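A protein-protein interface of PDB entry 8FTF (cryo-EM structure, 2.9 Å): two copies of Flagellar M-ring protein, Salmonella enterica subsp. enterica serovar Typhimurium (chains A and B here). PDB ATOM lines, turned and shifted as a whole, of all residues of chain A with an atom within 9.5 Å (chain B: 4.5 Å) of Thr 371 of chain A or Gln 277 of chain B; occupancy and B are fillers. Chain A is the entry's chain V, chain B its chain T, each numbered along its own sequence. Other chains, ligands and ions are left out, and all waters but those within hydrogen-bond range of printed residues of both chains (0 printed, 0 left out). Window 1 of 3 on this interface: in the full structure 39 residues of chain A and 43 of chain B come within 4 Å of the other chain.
O of Arg 370 of chain A touches O of Thr 278 of chain B, at 3.6 Å.
O of Arg 370 of chain A touches CA of Glu 279 of chain B, at 3.7 Å.
Thr 371 of chain A touches Gln 277 of chain B (CG2 to NE2, 3.5 Å).
Thr 278 of chain B touches Thr 371 of chain A (O to CA, 3.0 Å).
Thr 371 of chain A touches Glu 279 of chain B.
Glu 276 of chain B touches Ile 372 of chain A (O to O, 3.7 Å).
Ile 372 of chain A touches Gln 277 of chain B.
O of Glu 276 of chain B touches CA of Arg 373 of chain A, 2.8 Å away.
N of Glu 276 of chain B sits at hydrogen-bond distance from O of His 374 of chain A (2.8 Å).
The backbone NH of Thr 278 of chain B lies within hydrogen-bond range of the backbone carbonyl oxygen of Ile 372 of chain A.
Positions printed for both chains: 278, 279, 373, 374 and 375.
Of the 10 pairs that touch across the chains among the printed residues, none has its exchanged pair printed and touching as well.
Of the 14 printed residues of chain A, 5 touch a printed residue of chain B.
Of the 8 printed residues of chain B, 4 touch a printed residue of chain A.
Printed residues of chain B that touch a printed residue of chain A: Glu 276, Gln 277, Thr 278 and Glu 279.
Among the printed residues, no Asp or Glu carboxylate lies within 4 Å of a Lys or Arg side-chain nitrogen of the other chain.
The side-chain carboxylate (OE2) of Glu 279 of chain B sits at hydrogen-bond distance from the side-chain amide nitrogen (NE2) of Gln 277 of chain B (3.2 Å).
The backbone carbonyl oxygen (O) of Gln 277 of chain B is in hydrogen-bond range of the backbone NH (N) of Thr 375 of chain B, at 3.0 Å.
The side-chain hydroxyl (OG1) of Thr 278 of chain B lies within hydrogen-bond range of a ring nitrogen (ND1) of His 374 of chain B (3.5 Å).
The backbone carbonyl oxygen (O) of Arg 373 of chain B is in hydrogen-bond range of the backbone NH (N) of Glu 279 of chain B (3.0 Å).
The backbone NH (N) of Glu 279 of chain A lies within hydrogen-bond range of the backbone carbonyl oxygen (O) of Arg 373 of chain A, 3.0 Å away.
The backbone NH (N) of His 281 of chain A is in hydrogen-bond range of the backbone carbonyl oxygen (O) of Thr 371 of chain A (3.1 Å).
Of chain B, only Gln 277 (3.5 Å), Thr 278 (3.0 Å) and Glu 279 (3.8 Å) come within 4 Å of Thr 371 of chain A.
Of chain A, only Thr 371 and Ile 372 come within 4 Å of Gln 277 of chain B.
Thr 278 of chain B touches just these residues of chain A: Arg 370, Thr 371 and Ile 372.
No residue of chain A comes within 4 Å of His 374 of chain B.
Of the printed residues of chain B, His 374 of chain A touches Glu 276.
Of the printed residues of chain A, Glu 279 of chain B touches Arg 370 (3.7 Å) and Thr 371 (3.8 Å).
Of the printed residues of chain B, Arg 370 of chain A touches Thr 278 and Glu 279.
Printed residues of chain B within 4 Å of Ile 372 of chain A: Glu 276 (3.7 Å), Gln 277 (3.0 Å) and Thr 278 (2.8 Å).
Tyr 282 of chain A touches none of the printed residues of chain B.
Thr 278 of chain A touches none of the printed residues of chain B.
The nearest residue of chain A that does not touch Gln 277 of chain B is Arg 373 of chain A (4.1 Å).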
ATOM      1  N   THR A 278     -19.274  -0.694  23.128  1.00  0.00           N
ATOM      2  CA  THR A 278     -18.562  -1.959  23.235  1.00  0.00           C
ATOM      3  C   THR A 278     -19.425  -3.053  22.628  1.00  0.00           C
ATOM      4  O   THR A 278     -20.609  -3.167  22.959  1.00  0.00           O
ATOM      5  CB  THR A 278     -18.227  -2.293  24.692  1.00  0.00           C
ATOM      6  OG1 THR A 278     -17.703  -1.129  25.343  1.00  0.00           O
ATOM      7  CG2 THR A 278     -17.199  -3.411  24.759  1.00  0.00           C
ATOM      8  N   GLU A 279     -18.833  -3.854  21.746  1.00  0.00           N
ATOM      9  CA  GLU A 279     -19.547  -4.906  21.034  1.00  0.00           C
ATOM     10  C   GLU A 279     -18.854  -6.238  21.267  1.00  0.00           C
ATOM     11  O   GLU A 279     -17.621  -6.319  21.224  1.00  0.00           O
ATOM     12  CB  GLU A 279     -19.621  -4.603  19.537  1.00  0.00           C
ATOM     13  CG  GLU A 279     -20.450  -3.379  19.191  1.00  0.00           C
ATOM     14  CD  GLU A 279     -20.431  -3.064  17.708  1.00  0.00           C
ATOM     15  OE1 GLU A 279     -19.669  -3.721  16.970  1.00  0.00           O
ATOM     16  OE2 GLU A 279     -21.179  -2.161  17.281  1.00  0.00           O
ATOM     17  N   GLU A 280     -19.645  -7.277  21.512  1.00  0.00           N
ATOM     18  CA  GLU A 280     -19.144  -8.632  21.709  1.00  0.00           C
ATOM     19  C   GLU A 280     -19.991  -9.588  20.883  1.00  0.00           C
ATOM     20  O   GLU A 280     -21.218  -9.616  21.023  1.00  0.00           O
ATOM     21  CB  GLU A 280     -19.177  -9.016  23.190  1.00  0.00           C
ATOM     22  CG  GLU A 280     -18.756 -10.443  23.482  1.00  0.00           C
ATOM     23  CD  GLU A 280     -18.432 -10.658  24.947  1.00  0.00           C
ATOM     24  OE1 GLU A 280     -18.085  -9.673  25.631  1.00  0.00           O
ATOM     25  OE2 GLU A 280     -18.524 -11.811  25.419  1.00  0.00           O
ATOM     26  N   HIS A 281     -19.338 -10.369  20.025  1.00  0.00           N
ATOM     27  CA  HIS A 281     -20.017 -11.241  19.078  1.00  0.00           C
ATOM     28  C   HIS A 281     -19.458 -12.653  19.180  1.00  0.00           C
ATOM     29  O   HIS A 281     -18.252 -12.836  19.370  1.00  0.00           O
ATOM     30  CB  HIS A 281     -19.863 -10.713  17.648  1.00  0.00           C
ATOM     31  CG  HIS A 281     -20.564 -11.543  16.619  1.00  0.00           C
ATOM     32  ND1 HIS A 281     -21.934 -11.548  16.473  1.00  0.00           N
ATOM     33  CD2 HIS A 281     -20.083 -12.398  15.684  1.00  0.00           C
ATOM     34  CE1 HIS A 281     -22.268 -12.367  15.492  1.00  0.00           C
ATOM     35  NE2 HIS A 281     -21.164 -12.896  14.997  1.00  0.00           N
ATOM     36  N   TYR A 282     -20.339 -13.642  19.055  1.00  0.00           N
ATOM     37  CA  TYR A 282     -19.966 -15.050  19.073  1.00  0.00           C
ATOM     38  C   TYR A 282     -20.408 -15.702  17.772  1.00  0.00           C
ATOM     39  O   TYR A 282     -21.547 -15.508  17.334  1.00  0.00           O
ATOM     40  CB  TYR A 282     -20.596 -15.781  20.262  1.00  0.00           C
ATOM     41  CG  TYR A 282     -19.986 -15.439  21.603  1.00  0.00           C
ATOM     42  CD1 TYR A 282     -20.200 -14.201  22.190  1.00  0.00           C
ATOM     43  CD2 TYR A 282     -19.199 -16.359  22.283  1.00  0.00           C
ATOM     44  CE1 TYR A 282     -19.648 -13.888  23.413  1.00  0.00           C
ATOM     45  CE2 TYR A 282     -18.642 -16.053  23.508  1.00  0.00           C
ATOM     46  CZ  TYR A 282     -18.867 -14.816  24.068  1.00  0.00           C
ATOM     47  OH  TYR A 282     -18.315 -14.504  25.289  1.00  0.00           O
ATOM     48  N   SER A 283     -19.512 -16.470  17.158  1.00  0.00           N
ATOM     49  CA  SER A 283     -19.864 -17.189  15.949  1.00  0.00           C
ATOM     50  C   SER A 283     -20.738 -18.397  16.286  1.00  0.00           C
ATOM     51  O   SER A 283     -20.476 -19.112  17.257  1.00  0.00           O
ATOM     52  CB  SER A 283     -18.609 -17.646  15.210  1.00  0.00           C
ATOM     53  OG  SER A 283     -17.792 -16.542  14.865  1.00  0.00           O
ATOM     54  N   VAL A 368     -15.713 -21.799  21.828  1.00  0.00           N
ATOM     55  CA  VAL A 368     -16.428 -20.908  20.922  1.00  0.00           C
ATOM     56  C   VAL A 368     -15.537 -19.733  20.550  1.00  0.00           C
ATOM     57  O   VAL A 368     -14.673 -19.320  21.331  1.00  0.00           O
ATOM     58  CB  VAL A 368     -17.746 -20.409  21.549  1.00  0.00           C
ATOM     59  CG1 VAL A 368     -18.753 -21.540  21.635  1.00  0.00           C
ATOM     60  CG2 VAL A 368     -17.487 -19.813  22.923  1.00  0.00           C
ATOM     61  N   ASP A 369     -15.753 -19.199  19.351  1.00  0.00           N
ATOM     62  CA  ASP A 369     -15.058 -17.997  18.918  1.00  0.00           C
ATOM     63  C   ASP A 369     -15.643 -16.771  19.611  1.00  0.00           C
ATOM     64  O   ASP A 369     -16.806 -16.757  20.024  1.00  0.00           O
ATOM     65  CB  ASP A 369     -15.162 -17.840  17.400  1.00  0.00           C
ATOM     66  CG  ASP A 369     -14.481 -18.968  16.650  1.00  0.00           C
ATOM     67  OD1 ASP A 369     -13.508 -19.540  17.186  1.00  0.00           O
ATOM     68  OD2 ASP A 369     -14.920 -19.284  15.525  1.00  0.00           O
ATOM     69  N   ARG A 370     -14.823 -15.730  19.735  1.00  0.00           N
ATOM     70  CA  ARG A 370     -15.212 -14.532  20.464  1.00  0.00           C
ATOM     71  C   ARG A 370     -14.464 -13.327  19.919  1.00  0.00           C
ATOM     72  O   ARG A 370     -13.250 -13.386  19.696  1.00  0.00           O
ATOM     73  CB  ARG A 370     -14.949 -14.702  21.965  1.00  0.00           C
ATOM     74  CG  ARG A 370     -15.374 -13.529  22.822  1.00  0.00           C
ATOM     75  CD  ARG A 370     -15.083 -13.803  24.288  1.00  0.00           C
ATOM     76  NE  ARG A 370     -13.657 -13.970  24.546  1.00  0.00           N
ATOM     77  CZ  ARG A 370     -12.806 -12.970  24.729  1.00  0.00           C
ATOM     78  NH1 ARG A 370     -13.200 -11.709  24.681  1.00  0.00           N
ATOM     79  NH2 ARG A 370     -11.527 -13.244  24.968  1.00  0.00           N
ATOM     80  N   THR A 371     -15.197 -12.236  19.709  1.00  0.00           N
ATOM     81  CA  THR A 371     -14.656 -11.009  19.139  1.00  0.00           C
ATOM     82  C   THR A 371     -15.159  -9.818  19.940  1.00  0.00           C
ATOM     83  O   THR A 371     -16.355  -9.729  20.235  1.00  0.00           O
ATOM     84  CB  THR A 371     -15.058 -10.868  17.666  1.00  0.00           C
ATOM     85  OG1 THR A 371     -14.654 -12.039  16.946  1.00  0.00           O
ATOM     86  CG2 THR A 371     -14.401  -9.651  17.045  1.00  0.00           C
ATOM     87  N   ILE A 372     -14.253  -8.907  20.292  1.00  0.00           N
ATOM     88  CA  ILE A 372     -14.588  -7.703  21.047  1.00  0.00           C
ATOM     89  C   ILE A 372     -13.981  -6.489  20.360  1.00  0.00           C
ATOM     90  O   ILE A 372     -12.768  -6.442  20.129  1.00  0.00           O
ATOM     91  CB  ILE A 372     -14.107  -7.791  22.507  1.00  0.00           C
ATOM     92  CG1 ILE A 372     -15.015  -8.711  23.319  1.00  0.00           C
ATOM     93  CG2 ILE A 372     -14.034  -6.407  23.137  1.00  0.00           C
ATOM     94  CD1 ILE A 372     -14.623  -8.814  24.777  1.00  0.00           C
ATOM     95  N   ARG A 373     -14.822  -5.496  20.074  1.00  0.00           N
ATOM     96  CA  ARG A 373     -14.409  -4.200  19.547  1.00  0.00           C
ATOM     97  C   ARG A 373     -14.847  -3.105  20.507  1.00  0.00           C
ATOM     98  O   ARG A 373     -16.006  -3.074  20.930  1.00  0.00           O
ATOM     99  CB  ARG A 373     -15.005  -3.940  18.154  1.00  0.00           C
ATOM    100  N   HIS A 374     -13.920  -2.212  20.844  1.00  0.00           N
ATOM    101  CA  HIS A 374     -14.192  -1.053  21.686  1.00  0.00           C
ATOM    102  C   HIS A 374     -14.008   0.198  20.840  1.00  0.00           C
ATOM    103  O   HIS A 374     -12.941   0.395  20.249  1.00  0.00           O
ATOM    104  CB  HIS A 374     -13.263  -1.029  22.904  1.00  0.00           C
ATOM    105  CG  HIS A 374     -13.484   0.142  23.811  1.00  0.00           C
ATOM    106  ND1 HIS A 374     -14.649   0.326  24.523  1.00  0.00           N
ATOM    107  CD2 HIS A 374     -12.681   1.186  24.132  1.00  0.00           C
ATOM    108  CE1 HIS A 374     -14.558   1.434  25.236  1.00  0.00           C
ATOM    109  NE2 HIS A 374     -13.373   1.975  25.018  1.00  0.00           N
ATOM    110  N   THR A 375     -15.041   1.034  20.779  1.00  0.00           N
ATOM    111  CA  THR A 375     -15.043   2.219  19.934  1.00  0.00           C
ATOM    112  C   THR A 375     -15.348   3.452  20.772  1.00  0.00           C
ATOM    113  O   THR A 375     -16.328   3.468  21.525  1.00  0.00           O
ATOM    114  CB  THR A 375     -16.066   2.090  18.802  1.00  0.00           C
ATOM    115  OG1 THR A 375     -15.777   0.923  18.023  1.00  0.00           O
ATOM    116  CG2 THR A 375     -16.024   3.316  17.903  1.00  0.00           C
ATOM    117  N   GLU B 276     -10.815  -0.651  18.698  1.00  0.00           N
ATOM    118  CA  GLU B 276      -9.999  -1.807  19.037  1.00  0.00           C
ATOM    119  C   GLU B 276     -10.800  -3.067  18.747  1.00  0.00           C
ATOM    120  O   GLU B 276     -12.033  -3.050  18.758  1.00  0.00           O
ATOM    121  CB  GLU B 276      -9.556  -1.788  20.506  1.00  0.00           C
ATOM    122  CG  GLU B 276      -8.594  -0.666  20.851  1.00  0.00           C
ATOM    123  CD  GLU B 276      -8.161  -0.697  22.303  1.00  0.00           C
ATOM    124  OE1 GLU B 276      -8.704  -1.523  23.068  1.00  0.00           O
ATOM    125  OE2 GLU B 276      -7.279   0.101  22.682  1.00  0.00           O
ATOM    126  N   GLN B 277     -10.090  -4.162  18.487  1.00  0.00           N
ATOM    127  CA  GLN B 277     -10.734  -5.415  18.125  1.00  0.00           C
ATOM    128  C   GLN B 277      -9.864  -6.589  18.543  1.00  0.00           C
ATOM    129  O   GLN B 277      -8.640  -6.557  18.379  1.00  0.00           O
ATOM    130  CB  GLN B 277     -11.012  -5.479  16.618  1.00  0.00           C
ATOM    131  CG  GLN B 277     -11.693  -6.757  16.161  1.00  0.00           C
ATOM    132  CD  GLN B 277     -12.327  -6.620  14.792  1.00  0.00           C
ATOM    133  OE1 GLN B 277     -11.896  -5.808  13.974  1.00  0.00           O
ATOM    134  NE2 GLN B 277     -13.356  -7.417  14.535  1.00  0.00           N
ATOM    135  N   THR B 278     -10.503  -7.624  19.085  1.00  0.00           N
ATOM    136  CA  THR B 278      -9.840  -8.870  19.445  1.00  0.00           C
ATOM    137  C   THR B 278     -10.629 -10.027  18.855  1.00  0.00           C
ATOM    138  O   THR B 278     -11.851 -10.095  19.020  1.00  0.00           O
ATOM    139  CB  THR B 278      -9.727  -9.025  20.966  1.00  0.00           C
ATOM    140  OG1 THR B 278      -9.279  -7.792  21.542  1.00  0.00           O
ATOM    141  CG2 THR B 278      -8.743 -10.131  21.315  1.00  0.00           C
ATOM    142  N   GLU B 279      -9.933 -10.931  18.170  1.00  0.00           N
ATOM    143  CA  GLU B 279     -10.559 -12.059  17.493  1.00  0.00           C
ATOM    144  C   GLU B 279      -9.935 -13.355  17.983  1.00  0.00           C
ATOM    145  O   GLU B 279      -8.711 -13.445  18.131  1.00  0.00           O
ATOM    146  CB  GLU B 279     -10.409 -11.939  15.975  1.00  0.00           C
ATOM    147  CG  GLU B 279     -11.153 -10.764  15.368  1.00  0.00           C
ATOM    148  CD  GLU B 279     -10.914 -10.632  13.876  1.00  0.00           C
ATOM    149  OE1 GLU B 279     -10.066 -11.376  13.341  1.00  0.00           O
ATOM    150  OE2 GLU B 279     -11.573  -9.784  13.239  1.00  0.00           O
ATOM    151  N   ARG B 373      -5.758 -12.778  17.312  1.00  0.00           N
ATOM    152  CA  ARG B 373      -5.246 -11.557  16.698  1.00  0.00           C
ATOM    153  C   ARG B 373      -5.795 -10.352  17.447  1.00  0.00           C
ATOM    154  O   ARG B 373      -7.002 -10.265  17.689  1.00  0.00           O
ATOM    155  CB  ARG B 373      -5.628 -11.467  15.213  1.00  0.00           C
ATOM    156  N   HIS B 374      -4.908  -9.427  17.806  1.00  0.00           N
ATOM    157  CA  HIS B 374      -5.273  -8.175  18.454  1.00  0.00           C
ATOM    158  C   HIS B 374      -4.943  -7.036  17.501  1.00  0.00           C
ATOM    159  O   HIS B 374      -3.798  -6.916  17.052  1.00  0.00           O
ATOM    160  CB  HIS B 374      -4.530  -8.006  19.783  1.00  0.00           C
ATOM    161  CG  HIS B 374      -4.855  -6.732  20.502  1.00  0.00           C
ATOM    162  ND1 HIS B 374      -6.108  -6.459  21.009  1.00  0.00           N
ATOM    163  CD2 HIS B 374      -4.085  -5.661  20.810  1.00  0.00           C
ATOM    164  CE1 HIS B 374      -6.097  -5.273  21.590  1.00  0.00           C
ATOM    165  NE2 HIS B 374      -4.882  -4.767  21.484  1.00  0.00           N
ATOM    166  N   THR B 375      -5.938  -6.210  17.190  1.00  0.00           N
ATOM    167  CA  THR B 375      -5.793  -5.136  16.217  1.00  0.00           C
ATOM    168  C   THR B 375      -6.189  -3.810  16.848  1.00  0.00           C
ATOM    169  O   THR B 375      -7.268  -3.698  17.442  1.00  0.00           O
ATOM    170  CB  THR B 375      -6.645  -5.398  14.972  1.00  0.00           C
ATOM    171  OG1 THR B 375      -6.271  -6.652  14.389  1.00  0.00           O
ATOM    172  CG2 THR B 375      -6.446  -4.291  13.949  1.00  0.00           C
ATOM    173  N   MET B 377      -6.708  -0.102  15.431  1.00  0.00           N
ATOM    174  CA  MET B 377      -6.807   0.572  14.147  1.00  0.00           C
ATOM    175  C   MET B 377      -6.255   1.991  14.227  1.00  0.00           C
ATOM    176  O   MET B 377      -6.064   2.557  15.306  1.00  0.00           O
ATOM    177  CB  MET B 377      -8.257   0.594  13.664  1.00  0.00           C
ATOM    178  CG  MET B 377      -8.797  -0.777  13.292  1.00  0.00           C
ATOM    179  SD  MET B 377     -10.563  -0.945  13.599  1.00  0.00           S
ATOM    180  CE  MET B 377     -10.752  -2.724  13.505  1.00  0.00           C
